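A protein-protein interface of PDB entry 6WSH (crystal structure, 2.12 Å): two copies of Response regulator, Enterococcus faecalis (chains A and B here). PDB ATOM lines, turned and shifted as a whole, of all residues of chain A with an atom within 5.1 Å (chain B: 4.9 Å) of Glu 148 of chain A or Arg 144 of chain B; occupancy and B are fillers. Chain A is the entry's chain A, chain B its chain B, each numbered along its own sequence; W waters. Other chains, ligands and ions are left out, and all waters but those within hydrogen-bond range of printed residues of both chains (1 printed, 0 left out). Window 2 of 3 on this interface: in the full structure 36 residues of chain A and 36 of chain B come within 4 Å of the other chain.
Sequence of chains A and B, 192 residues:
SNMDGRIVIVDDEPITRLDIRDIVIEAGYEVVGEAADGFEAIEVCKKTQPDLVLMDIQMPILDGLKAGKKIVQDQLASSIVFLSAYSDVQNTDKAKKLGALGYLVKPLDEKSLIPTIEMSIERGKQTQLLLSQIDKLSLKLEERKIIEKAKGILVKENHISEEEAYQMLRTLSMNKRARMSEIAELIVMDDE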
ATOM      1  N   LEU A 141     -24.744  -7.808  -9.913  1.00  0.00           N
ATOM      2  CA  LEU A 141     -23.397  -7.750 -10.462  1.00  0.00           C
ATOM      3  C   LEU A 141     -22.339  -8.193  -9.454  1.00  0.00           C
ATOM      4  O   LEU A 141     -21.381  -8.893  -9.827  1.00  0.00           O
ATOM      5  CB  LEU A 141     -23.117  -6.336 -10.970  1.00  0.00           C
ATOM      6  CG  LEU A 141     -21.944  -6.113 -11.911  1.00  0.00           C
ATOM      7  CD1 LEU A 141     -22.329  -6.634 -13.278  1.00  0.00           C
ATOM      8  CD2 LEU A 141     -21.603  -4.623 -11.983  1.00  0.00           C
ATOM      9  N   GLU A 143     -22.831 -10.334  -6.991  1.00  0.00           N
ATOM     10  CA  GLU A 143     -22.923 -11.789  -6.881  1.00  0.00           C
ATOM     11  C   GLU A 143     -22.187 -12.479  -8.026  1.00  0.00           C
ATOM     12  O   GLU A 143     -21.393 -13.414  -7.803  1.00  0.00           O
ATOM     13  CB  GLU A 143     -24.379 -12.253  -6.826  1.00  0.00           C
ATOM     14  CG  GLU A 143     -24.554 -13.783  -6.801  1.00  0.00           C
ATOM     15  CD  GLU A 143     -25.870 -14.229  -6.155  1.00  0.00           C
ATOM     16  OE1 GLU A 143     -25.791 -14.767  -5.022  1.00  0.00           O
ATOM     17  OE2 GLU A 143     -26.958 -14.056  -6.745  1.00  0.00           O
ATOM     18  N   ARG A 144     -22.427 -12.025  -9.263  1.00  0.00           N
ATOM     19  CA  ARG A 144     -21.665 -12.580 -10.378  1.00  0.00           C
ATOM     20  C   ARG A 144     -20.151 -12.428 -10.174  1.00  0.00           C
ATOM     21  O   ARG A 144     -19.380 -13.372 -10.420  1.00  0.00           O
ATOM     22  CB  ARG A 144     -22.088 -11.915 -11.697  1.00  0.00           C
ATOM     23  CG  ARG A 144     -23.452 -12.409 -12.260  1.00  0.00           C
ATOM     24  CD  ARG A 144     -23.908 -11.785 -13.623  1.00  0.00           C
ATOM     25  NE  ARG A 144     -24.985 -12.593 -14.189  1.00  0.00           N
ATOM     26  CZ  ARG A 144     -24.786 -13.696 -14.890  1.00  0.00           C
ATOM     27  NH1 ARG A 144     -23.555 -14.045 -15.224  1.00  0.00           N
ATOM     28  NH2 ARG A 144     -25.807 -14.418 -15.326  1.00  0.00           N
ATOM     29  N   LYS A 145     -19.701 -11.241  -9.756  1.00  0.00           N
ATOM     30  CA  LYS A 145     -18.265 -11.015  -9.585  1.00  0.00           C
ATOM     31  C   LYS A 145     -17.644 -11.893  -8.501  1.00  0.00           C
ATOM     32  O   LYS A 145     -16.562 -12.466  -8.698  1.00  0.00           O
ATOM     33  CB  LYS A 145     -18.022  -9.528  -9.309  1.00  0.00           C
ATOM     34  CG  LYS A 145     -18.102  -8.699 -10.597  1.00  0.00           C
ATOM     35  CD  LYS A 145     -17.703  -7.229 -10.444  1.00  0.00           C
ATOM     36  CE  LYS A 145     -18.615  -6.488  -9.480  1.00  0.00           C
ATOM     37  NZ  LYS A 145     -18.263  -5.041  -9.421  1.00  0.00           N
ATOM     38  N   ILE A 146     -18.293 -12.009  -7.347  1.00  0.00           N
ATOM     39  CA  ILE A 146     -17.701 -12.815  -6.288  1.00  0.00           C
ATOM     40  C   ILE A 146     -17.710 -14.292  -6.664  1.00  0.00           C
ATOM     41  O   ILE A 146     -16.774 -15.036  -6.326  1.00  0.00           O
ATOM     42  CB  ILE A 146     -18.403 -12.534  -4.944  1.00  0.00           C
ATOM     43  CG1 ILE A 146     -17.550 -13.027  -3.772  1.00  0.00           C
ATOM     44  CG2 ILE A 146     -19.777 -13.193  -4.916  1.00  0.00           C
ATOM     45  CD1 ILE A 146     -16.309 -12.198  -3.494  1.00  0.00           C
ATOM     46  N   ILE A 147     -18.754 -14.754  -7.356  1.00  0.00           N
ATOM     47  CA  ILE A 147     -18.725 -16.135  -7.835  1.00  0.00           C
ATOM     48  C   ILE A 147     -17.600 -16.354  -8.850  1.00  0.00           C
ATOM     49  O   ILE A 147     -16.932 -17.398  -8.834  1.00  0.00           O
ATOM     50  CB  ILE A 147     -20.101 -16.534  -8.403  1.00  0.00           C
ATOM     51  CG1 ILE A 147     -21.091 -16.623  -7.236  1.00  0.00           C
ATOM     52  CG2 ILE A 147     -20.029 -17.847  -9.140  1.00  0.00           C
ATOM     53  CD1 ILE A 147     -22.547 -16.747  -7.634  1.00  0.00           C
ATOM     54  N   GLU A 148     -17.419 -15.421  -9.792  1.00  0.00           N
ATOM     55  CA  GLU A 148     -16.293 -15.524 -10.727  1.00  0.00           C
ATOM     56  C   GLU A 148     -14.951 -15.608 -10.002  1.00  0.00           C
ATOM     57  O   GLU A 148     -14.102 -16.470 -10.312  1.00  0.00           O
ATOM     58  CB  GLU A 148     -16.326 -14.321 -11.684  1.00  0.00           C
ATOM     59  CG  GLU A 148     -15.212 -14.230 -12.728  1.00  0.00           C
ATOM     60  CD  GLU A 148     -15.439 -13.092 -13.740  1.00  0.00           C
ATOM     61  OE1 GLU A 148     -15.208 -13.328 -14.948  1.00  0.00           O
ATOM     62  OE2 GLU A 148     -15.868 -11.981 -13.343  1.00  0.00           O
ATOM     63  N   LYS A 149     -14.750 -14.734  -9.016  1.00  0.00           N
ATOM     64  CA  LYS A 149     -13.511 -14.733  -8.248  1.00  0.00           C
ATOM     65  C   LYS A 149     -13.304 -16.051  -7.499  1.00  0.00           C
ATOM     66  O   LYS A 149     -12.203 -16.628  -7.516  1.00  0.00           O
ATOM     67  CB  LYS A 149     -13.563 -13.556  -7.278  1.00  0.00           C
ATOM     68  CG  LYS A 149     -12.248 -13.019  -6.741  1.00  0.00           C
ATOM     69  CD  LYS A 149     -12.530 -11.807  -5.829  1.00  0.00           C
ATOM     70  CE  LYS A 149     -11.307 -10.908  -5.723  1.00  0.00           C
ATOM     71  NZ  LYS A 149     -11.133 -10.000  -6.908  1.00  0.00           N
ATOM     72  N   ALA A 150     -14.350 -16.537  -6.833  1.00  0.00           N
ATOM     73  CA  ALA A 150     -14.244 -17.814  -6.143  1.00  0.00           C
ATOM     74  C   ALA A 150     -13.931 -18.966  -7.087  1.00  0.00           C
ATOM     75  O   ALA A 150     -13.131 -19.855  -6.748  1.00  0.00           O
ATOM     76  CB  ALA A 150     -15.536 -18.111  -5.394  1.00  0.00           C
ATOM     77  N   LYS A 151     -14.607 -19.014  -8.235  1.00  0.00           N
ATOM     78  CA  LYS A 151     -14.285 -20.030  -9.223  1.00  0.00           C
ATOM     79  C   LYS A 151     -12.802 -20.005  -9.590  1.00  0.00           C
ATOM     80  O   LYS A 151     -12.150 -21.058  -9.665  1.00  0.00           O
ATOM     81  CB  LYS A 151     -15.131 -19.820 -10.475  1.00  0.00           C
ATOM     82  CG  LYS A 151     -16.597 -20.253 -10.350  1.00  0.00           C
ATOM     83  CD  LYS A 151     -17.473 -19.699 -11.496  1.00  0.00           C
ATOM     84  CE  LYS A 151     -16.964 -20.105 -12.887  1.00  0.00           C
ATOM     85  NZ  LYS A 151     -17.771 -19.465 -13.970  1.00  0.00           N
ATOM     86  N   GLY A 152     -12.258 -18.816  -9.881  1.00  0.00           N
ATOM     87  CA  GLY A 152     -10.854 -18.770 -10.245  1.00  0.00           C
ATOM     88  C   GLY A 152      -9.920 -19.188  -9.124  1.00  0.00           C
ATOM     89  O   GLY A 152      -8.892 -19.853  -9.362  1.00  0.00           O
ATOM     90  N   LEU B 139     -25.651  -2.173 -18.620  1.00  0.00           N
ATOM     91  CA  LEU B 139     -24.763  -2.631 -19.677  1.00  0.00           C
ATOM     92  C   LEU B 139     -23.821  -3.726 -19.194  1.00  0.00           C
ATOM     93  O   LEU B 139     -23.651  -4.758 -19.862  1.00  0.00           O
ATOM     94  CB  LEU B 139     -23.973  -1.449 -20.226  1.00  0.00           C
ATOM     95  CG  LEU B 139     -22.955  -1.621 -21.337  1.00  0.00           C
ATOM     96  CD1 LEU B 139     -23.668  -2.122 -22.574  1.00  0.00           C
ATOM     97  CD2 LEU B 139     -22.258  -0.293 -21.595  1.00  0.00           C
ATOM     98  N   LYS B 140     -23.151  -3.499 -18.064  1.00  0.00           N
ATOM     99  CA  LYS B 140     -22.240  -4.522 -17.562  1.00  0.00           C
ATOM    100  C   LYS B 140     -22.956  -5.845 -17.279  1.00  0.00           C
ATOM    101  O   LYS B 140     -22.447  -6.927 -17.625  1.00  0.00           O
ATOM    102  CB  LYS B 140     -21.558  -4.005 -16.304  1.00  0.00           C
ATOM    103  CG  LYS B 140     -20.542  -2.904 -16.603  1.00  0.00           C
ATOM    104  CD  LYS B 140     -19.912  -2.312 -15.339  1.00  0.00           C
ATOM    105  CE  LYS B 140     -18.857  -1.267 -15.726  1.00  0.00           C
ATOM    106  NZ  LYS B 140     -18.185  -0.659 -14.543  1.00  0.00           N
ATOM    107  N   LEU B 141     -24.151  -5.788 -16.690  1.00  0.00           N
ATOM    108  CA  LEU B 141     -24.874  -7.025 -16.411  1.00  0.00           C
ATOM    109  C   LEU B 141     -25.327  -7.743 -17.684  1.00  0.00           C
ATOM    110  O   LEU B 141     -25.183  -8.974 -17.796  1.00  0.00           O
ATOM    111  CB  LEU B 141     -26.073  -6.738 -15.510  1.00  0.00           C
ATOM    112  CG  LEU B 141     -26.915  -7.907 -15.018  1.00  0.00           C
ATOM    113  CD1 LEU B 141     -26.023  -8.873 -14.263  1.00  0.00           C
ATOM    114  CD2 LEU B 141     -28.029  -7.391 -14.117  1.00  0.00           C
ATOM    115  N   GLU B 142     -25.919  -7.012 -18.630  1.00  0.00           N
ATOM    116  CA  GLU B 142     -26.305  -7.655 -19.875  1.00  0.00           C
ATOM    117  C   GLU B 142     -25.104  -8.216 -20.640  1.00  0.00           C
ATOM    118  O   GLU B 142     -25.214  -9.274 -21.281  1.00  0.00           O
ATOM    119  CB  GLU B 142     -27.065  -6.658 -20.750  1.00  0.00           C
ATOM    120  CG  GLU B 142     -28.522  -6.446 -20.366  1.00  0.00           C
ATOM    121  CD  GLU B 142     -29.331  -7.706 -20.530  1.00  0.00           C
ATOM    122  OE1 GLU B 142     -29.192  -8.346 -21.597  1.00  0.00           O
ATOM    123  OE2 GLU B 142     -30.078  -8.061 -19.599  1.00  0.00           O
ATOM    124  N   GLU B 143     -23.967  -7.511 -20.641  1.00  0.00           N
ATOM    125  CA  GLU B 143     -22.779  -8.069 -21.281  1.00  0.00           C
ATOM    126  C   GLU B 143     -22.341  -9.366 -20.610  1.00  0.00           C
ATOM    127  O   GLU B 143     -22.018 -10.349 -21.299  1.00  0.00           O
ATOM    128  CB  GLU B 143     -21.666  -7.014 -21.289  1.00  0.00           C
ATOM    129  CG  GLU B 143     -22.014  -5.874 -22.257  1.00  0.00           C
ATOM    130  CD  GLU B 143     -20.878  -4.901 -22.592  1.00  0.00           C
ATOM    131  OE1 GLU B 143     -20.782  -4.506 -23.780  1.00  0.00           O
ATOM    132  OE2 GLU B 143     -20.071  -4.562 -21.697  1.00  0.00           O
ATOM    133  N   ARG B 144     -22.348  -9.411 -19.268  1.00  0.00           N
ATOM    134  CA  ARG B 144     -22.052 -10.683 -18.610  1.00  0.00           C
ATOM    135  C   ARG B 144     -23.042 -11.780 -19.015  1.00  0.00           C
ATOM    136  O   ARG B 144     -22.641 -12.929 -19.272  1.00  0.00           O
ATOM    137  CB  ARG B 144     -22.069 -10.505 -17.088  1.00  0.00           C
ATOM    138  CG  ARG B 144     -20.815  -9.847 -16.481  1.00  0.00           C
ATOM    139  CD  ARG B 144     -20.842  -9.624 -14.915  1.00  0.00           C
ATOM    140  NE  ARG B 144     -19.508  -9.146 -14.581  1.00  0.00           N
ATOM    141  CZ  ARG B 144     -18.474  -9.922 -14.296  1.00  0.00           C
ATOM    142  NH1 ARG B 144     -17.265  -9.394 -14.152  1.00  0.00           N
ATOM    143  NH2 ARG B 144     -18.636 -11.223 -14.169  1.00  0.00           N
ATOM    144  N   LYS B 145     -24.336 -11.456 -19.076  1.00  0.00           N
ATOM    145  CA  LYS B 145     -25.323 -12.478 -19.416  1.00  0.00           C
ATOM    146  C   LYS B 145     -25.131 -13.025 -20.830  1.00  0.00           C
ATOM    147  O   LYS B 145     -25.165 -14.246 -21.054  1.00  0.00           O
ATOM    148  CB  LYS B 145     -26.720 -11.892 -19.260  1.00  0.00           C
ATOM    149  CG  LYS B 145     -27.157 -11.694 -17.808  1.00  0.00           C
ATOM    150  CD  LYS B 145     -28.525 -10.999 -17.757  1.00  0.00           C
ATOM    151  CE  LYS B 145     -29.045 -10.931 -16.327  1.00  0.00           C
ATOM    152  NZ  LYS B 145     -30.414 -10.357 -16.238  1.00  0.00           N
ATOM    153  N   ILE B 146     -24.941 -12.139 -21.799  1.00  0.00           N
ATOM    154  CA  ILE B 146     -24.783 -12.598 -23.170  1.00  0.00           C
ATOM    155  C   ILE B 146     -23.482 -13.373 -23.339  1.00  0.00           C
ATOM    156  O   ILE B 146     -23.427 -14.358 -24.089  1.00  0.00           O
ATOM    157  CB  ILE B 146     -24.909 -11.405 -24.136  1.00  0.00           C
ATOM    158  CG1 ILE B 146     -25.175 -11.890 -25.560  1.00  0.00           C
ATOM    159  CG2 ILE B 146     -23.648 -10.566 -24.093  1.00  0.00           C
ATOM    160  CD1 ILE B 146     -26.597 -12.382 -25.822  1.00  0.00           C
ATOM    161  N   ILE B 147     -22.403 -12.926 -22.697  1.00  0.00           N
ATOM    162  CA  ILE B 147     -21.163 -13.692 -22.781  1.00  0.00           C
ATOM    163  C   ILE B 147     -21.318 -15.080 -22.154  1.00  0.00           C
ATOM    164  O   ILE B 147     -20.758 -16.066 -22.661  1.00  0.00           O
ATOM    165  CB  ILE B 147     -20.010 -12.902 -22.138  1.00  0.00           C
ATOM    166  CG1 ILE B 147     -19.662 -11.715 -23.036  1.00  0.00           C
ATOM    167  CG2 ILE B 147     -18.799 -13.793 -21.930  1.00  0.00           C
ATOM    168  CD1 ILE B 147     -18.717 -10.696 -22.420  1.00  0.00           C
ATOM    169  N   GLU B 148     -22.031 -15.184 -21.029  1.00  0.00           N
ATOM    170  CA  GLU B 148     -22.289 -16.499 -20.437  1.00  0.00           C
ATOM    171  C   GLU B 148     -23.092 -17.414 -21.361  1.00  0.00           C
ATOM    172  O   GLU B 148     -22.740 -18.601 -21.554  1.00  0.00           O
ATOM    173  CB  GLU B 148     -23.014 -16.272 -19.110  1.00  0.00           C
ATOM    174  CG  GLU B 148     -23.408 -17.478 -18.274  1.00  0.00           C
ATOM    175  CD  GLU B 148     -24.064 -17.027 -16.959  1.00  0.00           C
ATOM    176  OE1 GLU B 148     -25.278 -16.711 -16.984  1.00  0.00           O
ATOM    177  OE2 GLU B 148     -23.365 -16.950 -15.922  1.00  0.00           O
HETATM  178  O   HOH W   1     -20.725 -13.328 -14.995  1.00  0.00           O
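Of the 10 printed residues of chain B, 4 touch a printed residue of chain A. Printed residues of chain A that touch a printed residue of chain B: Leu 141, Arg 144, Lys 145 and Glu 148. Hydrophobic or aromatic side chains of chain A that line the printed part of chain B: Leu 141.
The guanidinium group of Arg 144 of chain A lies within salt-bridge range of the side-chain carboxylate of Glu 148 of chain B, at 2.9 Å. The side-chain carboxylate (OE2) of Glu 148 of chain A is in salt-bridge range of the guanidinium group (NH2) of Arg 144 of chain B (3.0 Å).
Of the printed residues of chain B, Leu 141 of chain A touches Leu 141 (3.96 Å) and Arg 144 (3.7 Å). Glu 143 of chain A touches none of the printed residues of chain B. Glu 148 of chain A touches one residue of chain B. Of the printed residues of chain A, Leu 141 of chain B touches Leu 141 and Arg 144. Glu 142 of chain B touches none of the printed residues of chain A. Arg 144 of chain B touches four residues of chain A. The nearest printed residue of chain B that does not touch Glu 148 of chain A is Ile 147 of chain B (7.9 Å). The nearest printed residue of chain A that does not touch Lys 145 of chain B is Leu 141 of chain A (7.8 Å).
Leu 141 of chain A touches Leu 141 of chain B (CD1 to N, 3.96 Å). Leu 141 of chain A touches Arg 144 of chain B. Arg 144 of chain A touches Leu 141 of chain B (CD to CD1, 3.7 Å). CD of Arg 144 of chain A touches CD of Arg 144 of chain B, at 3.97 Å. CG of Lys 145 of chain B touches NH2 of Arg 144 of chain A, at 3.9 Å. Arg 144 of chain B touches Lys 145 of chain A (NH1 to CG, 3.7 Å).
Leu 141 of chain A touches Arg 144 of chain B, and with the chains exchanged Arg 144 of chain A touches Leu 141 of chain B. Arg 144 of chain B touches its own counterpart, Arg 144 of chain A. Arg 144 of chain A touches Lys 145 of chain B, and with the chains exchanged Lys 145 of chain A touches Arg 144 of chain B. Arg 144 of chain A touches Glu 148 of chain B, and with the chains exchanged Glu 148 of chain A touches Arg 144 of chain B.
Water W1 lies within hydrogen-bond range of NH1 of Arg 144 of chain A (2.9 Å) and NH2 of Arg 144 of chain B (3.1 Å).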
